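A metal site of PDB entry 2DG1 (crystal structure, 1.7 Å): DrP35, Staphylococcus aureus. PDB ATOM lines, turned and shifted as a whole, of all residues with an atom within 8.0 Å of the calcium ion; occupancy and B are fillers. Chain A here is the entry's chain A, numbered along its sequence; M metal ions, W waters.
The backbone NH (N) of Ser 110 lies within hydrogen-bond range of the side-chain sulfur (SG) of Cys 136 (3.2 Å). The backbone NH (N) of Ser 110 sits at hydrogen-bond distance from the side-chain carboxylate (OD2) of Asp 107 (2.9 Å). OG1 of Thr 133 lies within hydrogen-bond range of O of Glu 129, 3.2 Å away. OG1 of Thr 111 sits at hydrogen-bond distance from N of Asp 107 (2.8 Å). The backbone carbonyl oxygen (O) of Ala 134 lies within hydrogen-bond range of the guanidinium group (NE) of Arg 154 (3.1 Å).
Thr 111 touches the calcium ion. Ala 134 touches the calcium ion. Within 4 Å of the calcium ion: Ser 110, Thr 111, Gly 112, Asp 130, Thr 133, Ala 134 and Tyr 135.
The calcium ion is bound by the backbone carbonyl oxygen of Ser 110 (2.3 Å), water W1 (2.4 Å), the backbone carbonyl oxygen of Asp 130 (2.5 Å), the backbone carbonyl oxygen of Gly 112 (2.5 Å), the backbone carbonyl oxygen of Thr 133 (2.5 Å) and the backbone carbonyl oxygen of Tyr 135 (2.5 Å).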
ATOM      1  N   TYR A 104      10.666   8.638 -32.898  1.00  0.00           N
ATOM      2  CA  TYR A 104      10.634   7.591 -31.896  1.00  0.00           C
ATOM      3  C   TYR A 104      11.405   7.950 -30.633  1.00  0.00           C
ATOM      4  O   TYR A 104      12.385   8.695 -30.665  1.00  0.00           O
ATOM      5  CB  TYR A 104      11.144   6.253 -32.468  1.00  0.00           C
ATOM      6  CG  TYR A 104      12.545   6.289 -33.025  1.00  0.00           C
ATOM      7  CD1 TYR A 104      12.792   6.749 -34.319  1.00  0.00           C
ATOM      8  CD2 TYR A 104      13.624   5.844 -32.260  1.00  0.00           C
ATOM      9  CE1 TYR A 104      14.079   6.761 -34.841  1.00  0.00           C
ATOM     10  CE2 TYR A 104      14.922   5.858 -32.775  1.00  0.00           C
ATOM     11  CZ  TYR A 104      15.140   6.317 -34.063  1.00  0.00           C
ATOM     12  OH  TYR A 104      16.408   6.309 -34.579  1.00  0.00           O
ATOM     13  N   LEU A 105      10.967   7.380 -29.513  1.00  0.00           N
ATOM     14  CA  LEU A 105      11.544   7.669 -28.213  1.00  0.00           C
ATOM     15  C   LEU A 105      12.705   6.765 -27.769  1.00  0.00           C
ATOM     16  O   LEU A 105      13.410   7.082 -26.816  1.00  0.00           O
ATOM     17  CB  LEU A 105      10.439   7.628 -27.163  1.00  0.00           C
ATOM     18  CG  LEU A 105       9.229   8.516 -27.493  1.00  0.00           C
ATOM     19  CD1 LEU A 105       8.114   8.274 -26.490  1.00  0.00           C
ATOM     20  CD2 LEU A 105       9.656   9.976 -27.492  1.00  0.00           C
ATOM     21  N   GLY A 106      12.888   5.649 -28.462  1.00  0.00           N
ATOM     22  CA  GLY A 106      13.965   4.749 -28.085  1.00  0.00           C
ATOM     23  C   GLY A 106      13.816   4.224 -26.664  1.00  0.00           C
ATOM     24  O   GLY A 106      12.745   3.737 -26.298  1.00  0.00           O
ATOM     25  N   ASP A 107      14.876   4.329 -25.874  1.00  0.00           N
ATOM     26  CA  ASP A 107      14.840   3.847 -24.491  1.00  0.00           C
ATOM     27  C   ASP A 107      14.318   4.882 -23.507  1.00  0.00           C
ATOM     28  O   ASP A 107      14.442   4.712 -22.287  1.00  0.00           O
ATOM     29  CB  ASP A 107      16.225   3.374 -24.055  1.00  0.00           C
ATOM     30  CG  ASP A 107      17.240   4.514 -23.973  1.00  0.00           C
ATOM     31  OD1 ASP A 107      18.380   4.254 -23.549  1.00  0.00           O
ATOM     32  OD2 ASP A 107      16.897   5.659 -24.348  1.00  0.00           O
ATOM     33  N   LYS A 109      15.521   7.518 -22.677  1.00  0.00           N
ATOM     34  CA  LYS A 109      16.608   8.241 -22.035  1.00  0.00           C
ATOM     35  C   LYS A 109      17.456   9.022 -23.037  1.00  0.00           C
ATOM     36  O   LYS A 109      17.819  10.180 -22.789  1.00  0.00           O
ATOM     37  CB  LYS A 109      17.488   7.278 -21.252  1.00  0.00           C
ATOM     38  CG  LYS A 109      16.762   6.544 -20.135  1.00  0.00           C
ATOM     39  CD  LYS A 109      17.706   5.630 -19.383  1.00  0.00           C
ATOM     40  CE  LYS A 109      16.991   4.899 -18.258  1.00  0.00           C
ATOM     41  NZ  LYS A 109      17.931   4.013 -17.520  1.00  0.00           N
ATOM     42  N   SER A 110      17.792   8.399 -24.158  1.00  0.00           N
ATOM     43  CA  SER A 110      18.604   9.097 -25.150  1.00  0.00           C
ATOM     44  C   SER A 110      18.648   8.453 -26.534  1.00  0.00           C
ATOM     45  O   SER A 110      19.106   9.093 -27.474  1.00  0.00           O
ATOM     46  CB  SER A 110      20.037   9.225 -24.648  1.00  0.00           C
ATOM     47  OG  SER A 110      20.738   7.998 -24.777  1.00  0.00           O
ATOM     48  N   THR A 111      18.177   7.223 -26.669  1.00  0.00           N
ATOM     49  CA  THR A 111      18.259   6.545 -27.961  1.00  0.00           C
ATOM     50  C   THR A 111      17.101   6.751 -28.929  1.00  0.00           C
ATOM     51  O   THR A 111      16.829   5.885 -29.767  1.00  0.00           O
ATOM     52  CB  THR A 111      18.501   5.039 -27.777  1.00  0.00           C
ATOM     53  OG1 THR A 111      17.371   4.425 -27.153  1.00  0.00           O
ATOM     54  CG2 THR A 111      19.742   4.813 -26.913  1.00  0.00           C
ATOM     55  N   GLY A 112      16.431   7.886 -28.821  1.00  0.00           N
ATOM     56  CA  GLY A 112      15.341   8.186 -29.734  1.00  0.00           C
ATOM     57  C   GLY A 112      15.915   8.840 -30.975  1.00  0.00           C
ATOM     58  O   GLY A 112      17.121   9.033 -31.070  1.00  0.00           O
ATOM     59  N   GLY A 113      15.051   9.202 -31.919  1.00  0.00           N
ATOM     60  CA  GLY A 113      15.516   9.839 -33.147  1.00  0.00           C
ATOM     61  C   GLY A 113      14.387   9.930 -34.153  1.00  0.00           C
ATOM     62  O   GLY A 113      13.215   9.903 -33.783  1.00  0.00           O
ATOM     63  N   ILE A 114      14.734  10.035 -35.427  1.00  0.00           N
ATOM     64  CA  ILE A 114      13.719  10.106 -36.481  1.00  0.00           C
ATOM     65  C   ILE A 114      14.200   9.374 -37.723  1.00  0.00           C
ATOM     66  O   ILE A 114      15.315   9.606 -38.189  1.00  0.00           O
ATOM     67  CB  ILE A 114      13.420  11.569 -36.926  1.00  0.00           C
ATOM     68  CG1 ILE A 114      12.860  12.375 -35.763  1.00  0.00           C
ATOM     69  CG2 ILE A 114      12.418  11.553 -38.091  1.00  0.00           C
ATOM     70  CD1 ILE A 114      12.566  13.830 -36.126  1.00  0.00           C
ATOM     71  N   ILE A 128      17.434  11.578 -38.217  1.00  0.00           N
ATOM     72  CA  ILE A 128      18.121  12.004 -37.011  1.00  0.00           C
ATOM     73  C   ILE A 128      18.575  10.677 -36.411  1.00  0.00           C
ATOM     74  O   ILE A 128      17.757   9.906 -35.899  1.00  0.00           O
ATOM     75  CB  ILE A 128      17.191  12.711 -35.992  1.00  0.00           C
ATOM     76  CG1 ILE A 128      16.647  14.022 -36.584  1.00  0.00           C
ATOM     77  CG2 ILE A 128      17.961  12.982 -34.704  1.00  0.00           C
ATOM     78  CD1 ILE A 128      17.711  15.040 -36.923  1.00  0.00           C
ATOM     79  N   GLU A 129      19.874  10.412 -36.498  1.00  0.00           N
ATOM     80  CA  GLU A 129      20.449   9.171 -35.995  1.00  0.00           C
ATOM     81  C   GLU A 129      20.177   9.057 -34.486  1.00  0.00           C
ATOM     82  O   GLU A 129      20.218  10.062 -33.764  1.00  0.00           O
ATOM     83  CB  GLU A 129      21.948   9.159 -36.315  1.00  0.00           C
ATOM     84  CG  GLU A 129      22.637   7.815 -36.207  1.00  0.00           C
ATOM     85  CD  GLU A 129      23.125   7.535 -34.808  1.00  0.00           C
ATOM     86  OE1 GLU A 129      23.420   8.517 -34.096  1.00  0.00           O
ATOM     87  OE2 GLU A 129      23.236   6.364 -34.429  1.00  0.00           O
ATOM     88  N   ASP A 130      19.907   7.839 -34.031  1.00  0.00           N
ATOM     89  CA  ASP A 130      19.549   7.601 -32.630  1.00  0.00           C
ATOM     90  C   ASP A 130      20.603   7.581 -31.520  1.00  0.00           C
ATOM     91  O   ASP A 130      20.382   8.144 -30.450  1.00  0.00           O
ATOM     92  CB  ASP A 130      18.705   6.328 -32.535  1.00  0.00           C
ATOM     93  CG  ASP A 130      19.416   5.096 -33.099  1.00  0.00           C
ATOM     94  OD1 ASP A 130      20.356   5.263 -33.913  1.00  0.00           O
ATOM     95  OD2 ASP A 130      19.034   3.969 -32.731  1.00  0.00           O
ATOM     96  N   LEU A 131      21.745   6.946 -31.765  1.00  0.00           N
ATOM     97  CA  LEU A 131      22.777   6.842 -30.739  1.00  0.00           C
ATOM     98  C   LEU A 131      23.771   7.988 -30.603  1.00  0.00           C
ATOM     99  O   LEU A 131      24.332   8.183 -29.522  1.00  0.00           O
ATOM    100  CB  LEU A 131      23.553   5.531 -30.920  1.00  0.00           C
ATOM    101  CG  LEU A 131      22.719   4.242 -30.938  1.00  0.00           C
ATOM    102  CD1 LEU A 131      23.651   3.053 -31.126  1.00  0.00           C
ATOM    103  CD2 LEU A 131      21.927   4.107 -29.651  1.00  0.00           C
ATOM    104  N   SER A 132      23.996   8.744 -31.674  1.00  0.00           N
ATOM    105  CA  SER A 132      24.954   9.842 -31.637  1.00  0.00           C
ATOM    106  C   SER A 132      24.467  11.095 -30.902  1.00  0.00           C
ATOM    107  O   SER A 132      25.283  11.927 -30.486  1.00  0.00           O
ATOM    108  CB  SER A 132      25.384  10.225 -33.054  1.00  0.00           C
ATOM    109  OG  SER A 132      24.286  10.744 -33.796  1.00  0.00           O
ATOM    110  N   THR A 133      23.156  11.228 -30.749  1.00  0.00           N
ATOM    111  CA  THR A 133      22.597  12.380 -30.046  1.00  0.00           C
ATOM    112  C   THR A 133      21.678  11.907 -28.917  1.00  0.00           C
ATOM    113  O   THR A 133      21.160  10.791 -28.948  1.00  0.00           O
ATOM    114  CB  THR A 133      21.820  13.317 -30.987  1.00  0.00           C
ATOM    115  OG1 THR A 133      21.227  12.556 -32.041  1.00  0.00           O
ATOM    116  CG2 THR A 133      22.746  14.370 -31.564  1.00  0.00           C
ATOM    117  N   ALA A 134      21.469  12.773 -27.931  1.00  0.00           N
ATOM    118  CA  ALA A 134      20.653  12.425 -26.769  1.00  0.00           C
ATOM    119  C   ALA A 134      19.152  12.579 -26.915  1.00  0.00           C
ATOM    120  O   ALA A 134      18.415  12.315 -25.967  1.00  0.00           O
ATOM    121  CB  ALA A 134      21.131  13.221 -25.556  1.00  0.00           C
ATOM    122  N   TYR A 135      18.680  12.985 -28.091  1.00  0.00           N
ATOM    123  CA  TYR A 135      17.241  13.177 -28.285  1.00  0.00           C
ATOM    124  C   TYR A 135      16.378  11.926 -28.232  1.00  0.00           C
ATOM    125  O   TYR A 135      16.779  10.854 -28.673  1.00  0.00           O
ATOM    126  CB  TYR A 135      16.949  13.832 -29.638  1.00  0.00           C
ATOM    127  CG  TYR A 135      17.806  15.014 -30.008  1.00  0.00           C
ATOM    128  CD1 TYR A 135      18.674  14.940 -31.099  1.00  0.00           C
ATOM    129  CD2 TYR A 135      17.737  16.203 -29.286  1.00  0.00           C
ATOM    130  CE1 TYR A 135      19.443  16.034 -31.470  1.00  0.00           C
ATOM    131  CE2 TYR A 135      18.506  17.307 -29.658  1.00  0.00           C
ATOM    132  CZ  TYR A 135      19.356  17.213 -30.743  1.00  0.00           C
ATOM    133  OH  TYR A 135      20.127  18.287 -31.110  1.00  0.00           O
ATOM    134  N   CYS A 136      15.166  12.103 -27.703  1.00  0.00           N
ATOM    135  CA  CYS A 136      14.128  11.071 -27.665  1.00  0.00           C
ATOM    136  C   CYS A 136      13.013  11.936 -28.255  1.00  0.00           C
ATOM    137  O   CYS A 136      12.431  12.778 -27.579  1.00  0.00           O
ATOM    138  CB  CYS A 136      13.802  10.656 -26.241  1.00  0.00           C
ATOM    139  SG  CYS A 136      15.097   9.637 -25.483  1.00  0.00           S
ATOM    140  N   ILE A 137      12.750  11.731 -29.543  1.00  0.00           N
ATOM    141  CA  ILE A 137      11.793  12.545 -30.277  1.00  0.00           C
ATOM    142  C   ILE A 137      10.367  12.038 -30.338  1.00  0.00           C
ATOM    143  O   ILE A 137      10.099  10.940 -30.829  1.00  0.00           O
ATOM    144  CB  ILE A 137      12.342  12.794 -31.694  1.00  0.00           C
ATOM    145  CG1 ILE A 137      13.787  13.311 -31.576  1.00  0.00           C
ATOM    146  CG2 ILE A 137      11.466  13.794 -32.442  1.00  0.00           C
ATOM    147  CD1 ILE A 137      14.509  13.465 -32.905  1.00  0.00           C
ATOM    148  N   ASP A 152      11.737  17.234 -28.086  1.00  0.00           N
ATOM    149  CA  ASP A 152      12.636  16.346 -27.350  1.00  0.00           C
ATOM    150  C   ASP A 152      11.859  15.954 -26.096  1.00  0.00           C
ATOM    151  O   ASP A 152      11.681  16.760 -25.177  1.00  0.00           O
ATOM    152  CB  ASP A 152      13.932  17.069 -27.003  1.00  0.00           C
ATOM    153  CG  ASP A 152      15.014  16.138 -26.499  1.00  0.00           C
ATOM    154  OD1 ASP A 152      14.801  14.906 -26.504  1.00  0.00           O
ATOM    155  OD2 ASP A 152      16.078  16.643 -26.084  1.00  0.00           O
ATOM    156  N   ARG A 154      12.054  14.380 -23.133  1.00  0.00           N
ATOM    157  CA  ARG A 154      12.919  13.917 -22.049  1.00  0.00           C
ATOM    158  C   ARG A 154      12.715  14.670 -20.736  1.00  0.00           C
ATOM    159  O   ARG A 154      12.262  15.807 -20.719  1.00  0.00           O
ATOM    160  CB  ARG A 154      14.393  14.040 -22.469  1.00  0.00           C
ATOM    161  CG  ARG A 154      14.804  13.088 -23.590  1.00  0.00           C
ATOM    162  CD  ARG A 154      16.320  13.089 -23.761  1.00  0.00           C
ATOM    163  NE  ARG A 154      16.819  14.353 -24.286  1.00  0.00           N
ATOM    164  CZ  ARG A 154      17.900  14.969 -23.810  1.00  0.00           C
ATOM    165  NH1 ARG A 154      18.300  16.112 -24.349  1.00  0.00           N
ATOM    166  NH2 ARG A 154      18.571  14.452 -22.796  1.00  0.00           N
HETATM  167 CA    CA M   1      18.921   9.939 -29.629  1.00  0.00          CA
HETATM  168  O   HOH W   1      19.323  11.282 -31.519  1.00  0.00           O
